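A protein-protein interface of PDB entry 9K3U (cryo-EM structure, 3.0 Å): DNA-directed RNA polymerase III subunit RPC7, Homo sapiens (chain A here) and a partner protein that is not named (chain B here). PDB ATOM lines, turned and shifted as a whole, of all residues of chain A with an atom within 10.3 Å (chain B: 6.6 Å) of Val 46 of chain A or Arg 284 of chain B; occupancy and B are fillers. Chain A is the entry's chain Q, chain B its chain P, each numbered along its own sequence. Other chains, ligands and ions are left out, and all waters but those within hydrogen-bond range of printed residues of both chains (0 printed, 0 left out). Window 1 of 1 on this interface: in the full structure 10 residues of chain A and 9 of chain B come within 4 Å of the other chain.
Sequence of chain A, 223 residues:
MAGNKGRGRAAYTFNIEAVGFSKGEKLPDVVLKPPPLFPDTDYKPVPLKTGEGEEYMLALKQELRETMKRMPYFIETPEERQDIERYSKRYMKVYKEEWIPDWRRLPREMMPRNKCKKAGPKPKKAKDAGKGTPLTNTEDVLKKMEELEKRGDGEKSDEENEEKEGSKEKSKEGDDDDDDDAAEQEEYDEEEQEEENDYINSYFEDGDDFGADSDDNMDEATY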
ATOM      1  N   ASP A  42       7.282  -0.408  10.813  1.00  0.00           N
ATOM      2  CA  ASP A  42       6.736   0.929  10.623  1.00  0.00           C
ATOM      3  C   ASP A  42       7.809   2.007  10.547  1.00  0.00           C
ATOM      4  O   ASP A  42       7.481   3.161  10.250  1.00  0.00           O
ATOM      5  CB  ASP A  42       5.757   1.263  11.752  1.00  0.00           C
ATOM      6  CG  ASP A  42       6.382   1.122  13.126  1.00  0.00           C
ATOM      7  OD1 ASP A  42       7.513   0.605  13.215  1.00  0.00           O
ATOM      8  OD2 ASP A  42       5.737   1.530  14.118  1.00  0.00           O
ATOM      9  N   TYR A  43       9.070   1.668  10.805  1.00  0.00           N
ATOM     10  CA  TYR A  43      10.181   2.605  10.707  1.00  0.00           C
ATOM     11  C   TYR A  43      10.999   2.285   9.464  1.00  0.00           C
ATOM     12  O   TYR A  43      11.392   1.132   9.255  1.00  0.00           O
ATOM     13  CB  TYR A  43      11.068   2.542  11.953  1.00  0.00           C
ATOM     14  CG  TYR A  43      10.381   2.996  13.221  1.00  0.00           C
ATOM     15  CD1 TYR A  43      10.252   4.345  13.519  1.00  0.00           C
ATOM     16  CD2 TYR A  43       9.871   2.073  14.125  1.00  0.00           C
ATOM     17  CE1 TYR A  43       9.627   4.764  14.679  1.00  0.00           C
ATOM     18  CE2 TYR A  43       9.246   2.483  15.287  1.00  0.00           C
ATOM     19  CZ  TYR A  43       9.126   3.829  15.559  1.00  0.00           C
ATOM     20  OH  TYR A  43       8.504   4.242  16.716  1.00  0.00           O
ATOM     21  N   LYS A  44      11.253   3.306   8.642  1.00  0.00           N
ATOM     22  CA  LYS A  44      12.017   3.142   7.419  1.00  0.00           C
ATOM     23  C   LYS A  44      13.409   3.749   7.571  1.00  0.00           C
ATOM     24  O   LYS A  44      13.606   4.669   8.372  1.00  0.00           O
ATOM     25  CB  LYS A  44      11.309   3.804   6.230  1.00  0.00           C
ATOM     26  CG  LYS A  44       9.888   3.304   5.983  1.00  0.00           C
ATOM     27  CD  LYS A  44       9.836   1.804   5.701  1.00  0.00           C
ATOM     28  CE  LYS A  44      10.601   1.435   4.439  1.00  0.00           C
ATOM     29  NZ  LYS A  44      10.455  -0.007   4.102  1.00  0.00           N
ATOM     30  N   PRO A  45      14.400   3.260   6.822  1.00  0.00           N
ATOM     31  CA  PRO A  45      15.744   3.838   6.923  1.00  0.00           C
ATOM     32  C   PRO A  45      15.751   5.308   6.533  1.00  0.00           C
ATOM     33  O   PRO A  45      15.014   5.739   5.641  1.00  0.00           O
ATOM     34  CB  PRO A  45      16.571   2.992   5.948  1.00  0.00           C
ATOM     35  CG  PRO A  45      15.801   1.732   5.774  1.00  0.00           C
ATOM     36  CD  PRO A  45      14.362   2.113   5.898  1.00  0.00           C
ATOM     37  N   VAL A  46      16.591   6.076   7.210  1.00  0.00           N
ATOM     38  CA  VAL A  46      16.725   7.504   6.891  1.00  0.00           C
ATOM     39  C   VAL A  46      17.410   7.646   5.537  1.00  0.00           C
ATOM     40  O   VAL A  46      18.383   6.921   5.263  1.00  0.00           O
ATOM     41  CB  VAL A  46      17.514   8.222   7.991  1.00  0.00           C
ATOM     42  CG1 VAL A  46      17.604   9.720   7.718  1.00  0.00           C
ATOM     43  CG2 VAL A  46      16.878   7.965   9.351  1.00  0.00           C
ATOM     44  N   PRO A  47      16.955   8.544   4.661  1.00  0.00           N
ATOM     45  CA  PRO A  47      17.591   8.664   3.343  1.00  0.00           C
ATOM     46  C   PRO A  47      19.058   9.051   3.457  1.00  0.00           C
ATOM     47  O   PRO A  47      19.504   9.604   4.464  1.00  0.00           O
ATOM     48  CB  PRO A  47      16.772   9.759   2.648  1.00  0.00           C
ATOM     49  CG  PRO A  47      16.110  10.510   3.753  1.00  0.00           C
ATOM     50  CD  PRO A  47      15.842   9.496   4.820  1.00  0.00           C
ATOM     51  N   LEU A  48      19.808   8.750   2.400  1.00  0.00           N
ATOM     52  CA  LEU A  48      21.236   9.017   2.391  1.00  0.00           C
ATOM     53  C   LEU A  48      21.505  10.519   2.325  1.00  0.00           C
ATOM     54  O   LEU A  48      20.729  11.298   1.767  1.00  0.00           O
ATOM     55  CB  LEU A  48      21.908   8.319   1.207  1.00  0.00           C
ATOM     56  CG  LEU A  48      21.963   6.788   1.220  1.00  0.00           C
ATOM     57  CD1 LEU A  48      22.599   6.275   2.507  1.00  0.00           C
ATOM     58  CD2 LEU A  48      20.582   6.181   1.024  1.00  0.00           C
ATOM     59  N   LYS A  49      22.631  10.918   2.910  1.00  0.00           N
ATOM     60  CA  LYS A  49      23.054  12.309   2.847  1.00  0.00           C
ATOM     61  C   LYS A  49      23.374  12.693   1.409  1.00  0.00           C
ATOM     62  O   LYS A  49      24.076  11.973   0.697  1.00  0.00           O
ATOM     63  CB  LYS A  49      24.277  12.533   3.736  1.00  0.00           C
ATOM     64  CG  LYS A  49      24.045  12.215   5.208  1.00  0.00           C
ATOM     65  CD  LYS A  49      25.332  12.306   6.021  1.00  0.00           C
ATOM     66  CE  LYS A  49      25.896  13.721   6.052  1.00  0.00           C
ATOM     67  NZ  LYS A  49      24.932  14.703   6.620  1.00  0.00           N
ATOM     68  N   THR A  50      22.855  13.840   0.985  1.00  0.00           N
ATOM     69  CA  THR A  50      23.060  14.349  -0.361  1.00  0.00           C
ATOM     70  C   THR A  50      24.103  15.459  -0.344  1.00  0.00           C
ATOM     71  O   THR A  50      24.220  16.220   0.620  1.00  0.00           O
ATOM     72  CB  THR A  50      21.752  14.875  -0.960  1.00  0.00           C
ATOM     73  OG1 THR A  50      21.260  15.961  -0.164  1.00  0.00           O
ATOM     74  CG2 THR A  50      20.704  13.774  -1.015  1.00  0.00           C
ATOM     75  N   GLY A  51      24.863  15.544  -1.432  1.00  0.00           N
ATOM     76  CA  GLY A  51      25.878  16.570  -1.550  1.00  0.00           C
ATOM     77  C   GLY A  51      26.940  16.267  -2.586  1.00  0.00           C
ATOM     78  O   GLY A  51      27.184  15.104  -2.930  1.00  0.00           O
ATOM     79  N   GLU A  54      29.496  13.725  -1.276  1.00  0.00           N
ATOM     80  CA  GLU A  54      29.093  12.326  -1.356  1.00  0.00           C
ATOM     81  C   GLU A  54      29.094  11.837  -2.799  1.00  0.00           C
ATOM     82  O   GLU A  54      29.504  10.705  -3.081  1.00  0.00           O
ATOM     83  CB  GLU A  54      27.712  12.136  -0.729  1.00  0.00           C
ATOM     84  CG  GLU A  54      27.691  12.229   0.793  1.00  0.00           C
ATOM     85  CD  GLU A  54      27.939  13.633   1.302  1.00  0.00           C
ATOM     86  OE1 GLU A  54      28.063  14.558   0.472  1.00  0.00           O
ATOM     87  OE2 GLU A  54      28.009  13.816   2.537  1.00  0.00           O
ATOM     88  N   PRO B 278      23.961  14.613  13.430  1.00  0.00           N
ATOM     89  CA  PRO B 278      22.788  14.180  12.661  1.00  0.00           C
ATOM     90  C   PRO B 278      22.661  12.667  12.669  1.00  0.00           C
ATOM     91  O   PRO B 278      23.503  11.968  13.252  1.00  0.00           O
ATOM     92  CB  PRO B 278      23.069  14.709  11.245  1.00  0.00           C
ATOM     93  CG  PRO B 278      24.116  15.757  11.416  1.00  0.00           C
ATOM     94  CD  PRO B 278      24.936  15.325  12.585  1.00  0.00           C
ATOM     95  N   PRO B 279      21.620  12.122  12.039  1.00  0.00           N
ATOM     96  CA  PRO B 279      21.488  10.663  11.969  1.00  0.00           C
ATOM     97  C   PRO B 279      22.726  10.020  11.367  1.00  0.00           C
ATOM     98  O   PRO B 279      23.278  10.498  10.371  1.00  0.00           O
ATOM     99  CB  PRO B 279      20.256  10.462  11.081  1.00  0.00           C
ATOM    100  CG  PRO B 279      19.470  11.721  11.231  1.00  0.00           C
ATOM    101  CD  PRO B 279      20.481  12.815  11.410  1.00  0.00           C
ATOM    102  N   THR B 280      23.163   8.924  11.981  1.00  0.00           N
ATOM    103  CA  THR B 280      24.369   8.241  11.539  1.00  0.00           C
ATOM    104  C   THR B 280      24.115   7.499  10.226  1.00  0.00           C
ATOM    105  O   THR B 280      23.014   7.517   9.667  1.00  0.00           O
ATOM    106  CB  THR B 280      24.855   7.269  12.613  1.00  0.00           C
ATOM    107  OG1 THR B 280      23.827   6.312  12.899  1.00  0.00           O
ATOM    108  CG2 THR B 280      25.217   8.022  13.885  1.00  0.00           C
ATOM    109  N   GLY B 281      25.166   6.840   9.732  1.00  0.00           N
ATOM    110  CA  GLY B 281      25.068   6.120   8.473  1.00  0.00           C
ATOM    111  C   GLY B 281      24.443   4.748   8.578  1.00  0.00           C
ATOM    112  O   GLY B 281      23.859   4.271   7.597  1.00  0.00           O
ATOM    113  N   LEU B 282      24.549   4.098   9.739  1.00  0.00           N
ATOM    114  CA  LEU B 282      23.960   2.775   9.898  1.00  0.00           C
ATOM    115  C   LEU B 282      22.453   2.812   9.686  1.00  0.00           C
ATOM    116  O   LEU B 282      21.886   1.928   9.031  1.00  0.00           O
ATOM    117  CB  LEU B 282      24.291   2.217  11.283  1.00  0.00           C
ATOM    118  CG  LEU B 282      23.694   0.845  11.614  1.00  0.00           C
ATOM    119  CD1 LEU B 282      24.230  -0.223  10.674  1.00  0.00           C
ATOM    120  CD2 LEU B 282      23.969   0.481  13.063  1.00  0.00           C
ATOM    121  N   VAL B 283      21.785   3.832  10.231  1.00  0.00           N
ATOM    122  CA  VAL B 283      20.335   3.937  10.108  1.00  0.00           C
ATOM    123  C   VAL B 283      19.888   4.190   8.677  1.00  0.00           C
ATOM    124  O   VAL B 283      18.718   3.956   8.354  1.00  0.00           O
ATOM    125  CB  VAL B 283      19.798   5.059  11.020  1.00  0.00           C
ATOM    126  CG1 VAL B 283      20.246   4.838  12.457  1.00  0.00           C
ATOM    127  CG2 VAL B 283      20.249   6.425  10.517  1.00  0.00           C
ATOM    128  N   ARG B 284      20.786   4.662   7.814  1.00  0.00           N
ATOM    129  CA  ARG B 284      20.451   4.933   6.424  1.00  0.00           C
ATOM    130  C   ARG B 284      20.445   3.681   5.558  1.00  0.00           C
ATOM    131  O   ARG B 284      20.107   3.774   4.372  1.00  0.00           O
ATOM    132  CB  ARG B 284      21.432   5.956   5.843  1.00  0.00           C
ATOM    133  CG  ARG B 284      21.394   7.310   6.534  1.00  0.00           C
ATOM    134  CD  ARG B 284      22.314   8.308   5.853  1.00  0.00           C
ATOM    135  NE  ARG B 284      22.127   9.667   6.360  1.00  0.00           N
ATOM    136  CZ  ARG B 284      22.811  10.205   7.366  1.00  0.00           C
ATOM    137  NH1 ARG B 284      23.748   9.506   7.995  1.00  0.00           N
ATOM    138  NH2 ARG B 284      22.559  11.450   7.744  1.00  0.00           N
ATOM    139  N   ALA B 285      20.810   2.521   6.114  1.00  0.00           N
ATOM    140  CA  ALA B 285      20.807   1.268   5.376  1.00  0.00           C
ATOM    141  C   ALA B 285      19.754   0.319   5.937  1.00  0.00           C
ATOM    142  O   ALA B 285      19.575   0.254   7.158  1.00  0.00           O
ATOM    143  CB  ALA B 285      22.181   0.591   5.438  1.00  0.00           C
ATOM    144  N   PRO B 286      19.040  -0.424   5.085  1.00  0.00           N
ATOM    145  CA  PRO B 286      18.041  -1.368   5.610  1.00  0.00           C
ATOM    146  C   PRO B 286      18.623  -2.417   6.540  1.00  0.00           C
ATOM    147  O   PRO B 286      17.882  -2.977   7.360  1.00  0.00           O
ATOM    148  CB  PRO B 286      17.460  -2.010   4.343  1.00  0.00           C
ATOM    149  CG  PRO B 286      17.743  -1.039   3.252  1.00  0.00           C
ATOM    150  CD  PRO B 286      19.039  -0.387   3.612  1.00  0.00           C
ATOM    151  N   CYS B 287      19.923  -2.703   6.443  1.00  0.00           N
ATOM    152  CA  CYS B 287      20.516  -3.736   7.288  1.00  0.00           C
ATOM    153  C   CYS B 287      20.549  -3.318   8.749  1.00  0.00           C
ATOM    154  O   CYS B 287      20.379  -4.163   9.637  1.00  0.00           O
ATOM    155  CB  CYS B 287      21.929  -4.060   6.803  1.00  0.00           C
ATOM    156  SG  CYS B 287      22.038  -4.493   5.051  1.00  0.00           S
ATOM    157  N   LEU B 289      18.402  -1.382  10.354  1.00  0.00           N
ATOM    158  CA  LEU B 289      17.063  -1.298  10.922  1.00  0.00           C
ATOM    159  C   LEU B 289      16.253  -2.568  10.686  1.00  0.00           C
ATOM    160  O   LEU B 289      15.022  -2.531  10.772  1.00  0.00           O
ATOM    161  CB  LEU B 289      16.321  -0.093  10.341  1.00  0.00           C
ATOM    162  CG  LEU B 289      17.076   1.238  10.380  1.00  0.00           C
ATOM    163  CD1 LEU B 289      16.217   2.355   9.811  1.00  0.00           C
ATOM    164  CD2 LEU B 289      17.527   1.572  11.795  1.00  0.00           C
ATOM    165  N   TRP B 313      13.870  -0.570  -0.635  1.00  0.00           N
ATOM    166  CA  TRP B 313      14.643   0.637  -0.364  1.00  0.00           C
ATOM    167  C   TRP B 313      15.311   1.160  -1.629  1.00  0.00           C
ATOM    168  O   TRP B 313      15.444   2.375  -1.814  1.00  0.00           O
ATOM    169  CB  TRP B 313      15.679   0.351   0.724  1.00  0.00           C
ATOM    170  CG  TRP B 313      16.724   1.410   0.869  1.00  0.00           C
ATOM    171  CD1 TRP B 313      16.544   2.686   1.316  1.00  0.00           C
ATOM    172  CD2 TRP B 313      18.120   1.279   0.582  1.00  0.00           C
ATOM    173  NE1 TRP B 313      17.742   3.361   1.318  1.00  0.00           N
ATOM    174  CE2 TRP B 313      18.724   2.518   0.870  1.00  0.00           C
ATOM    175  CE3 TRP B 313      18.916   0.234   0.102  1.00  0.00           C
ATOM    176  CZ2 TRP B 313      20.089   2.741   0.700  1.00  0.00           C
ATOM    177  CZ3 TRP B 313      20.271   0.457  -0.068  1.00  0.00           C
ATOM    178  CH2 TRP B 313      20.843   1.700   0.230  1.00  0.00           C
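The backbone carbonyl oxygen (O) of Pro 47 of chain A lies within hydrogen-bond range of the guanidinium group (NE) of Arg 284 of chain B, 3.2 Å away.
The backbone NH of Val 46 of chain A lies within hydrogen-bond range of the backbone carbonyl oxygen of Val 283 of chain B, at 3.2 Å.
The backbone carbonyl oxygen (O) of Pro 279 of chain B lies within hydrogen-bond range of the guanidinium group (NH1) of Arg 284 of chain B, at 2.6 Å.
The guanidinium group (NH1) of Arg 284 of chain B sits at hydrogen-bond distance from the backbone carbonyl oxygen (O) of Thr 280 of chain B (2.7 Å).
Lys 44 of chain A touches Leu 289 of chain B (O to CD1, 3.8 Å).
O of Val 283 of chain B touches CA of Pro 45 of chain A (3.3 Å).
CB of Pro 45 of chain A touches O of Arg 284 of chain B, 3.9 Å away.
Pro 45 of chain A touches Pro 286 of chain B.
Leu 289 of chain B touches Pro 45 of chain A (CD1 to CA, 3.3 Å).
Val 46 of chain A touches Arg 284 of chain B.
CD1 of Leu 48 of chain A touches CB of Arg 284 of chain B, at 3.5 Å.
CZ2 of Trp 313 of chain B touches CD2 of Leu 48 of chain A, at 3.5 Å.
CG of Lys 49 of chain A touches NH2 of Arg 284 of chain B, at 3.0 Å.
Val 46 of chain A touches just these residues of chain B: Val 283 (3.2 Å) and Arg 284 (3.1 Å).
Of chain A, only Pro 45 (3.9 Å), Val 46 (3.1 Å), Pro 47 (3.2 Å), Leu 48 (3.5 Å) and Lys 49 (3.0 Å) come within 4 Å of Arg 284 of chain B.
No residue of chain A comes within 4 Å of Pro 279 of chain B.
Thr 280 of chain B touches none of the printed residues of chain A.
Of chain A, only Pro 45 (3.3 Å) and Val 46 (3.2 Å) come within 4 Å of Val 283 of chain B.
No residue of chain A comes within 4 Å of Ala 285 of chain B.
Printed residues of chain A within 4 Å of Trp 313 of chain B: Leu 48 (3.5 Å).
Of the printed residues of chain B, Pro 47 of chain A touches Arg 284.
Of the printed residues of chain A, Pro 286 of chain B touches Pro 45 (3.8 Å).
Printed residues of chain B within 4 Å of Lys 49 of chain A: Arg 284 (3.0 Å).
Printed residues of chain A within 4 Å of Leu 289 of chain B: Lys 44 (3.8 Å) and Pro 45 (3.3 Å).
Cys 287 of chain B touches none of the printed residues of chain A.
Leu 282 of chain B touches none of the printed residues of chain A.
The nearest residue of chain B that does not touch Val 46 of chain A is Pro 279 of chain B (4.3 Å).
The nearest printed residue of chain B that does not touch Pro 45 of chain A is Ala 285 of chain B (4.2 Å).
Hydrophobic or aromatic side chains of chain B within 4 Å of the printed part of chain A: Val 283, Leu 289 and Trp 313.
Of the 11 printed residues of chain A, 6 touch a printed residue of chain B.
Hydrophobic or aromatic side chains of chain A within 4 Å of the printed part of chain B: Pro 45, Val 46 and Leu 48.
Among the printed residues, 11 pairs touch across the chains.
Among the printed residues, no Asp or Glu carboxylate lies within 4 Å of a Lys or Arg side-chain nitrogen of the other chain.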
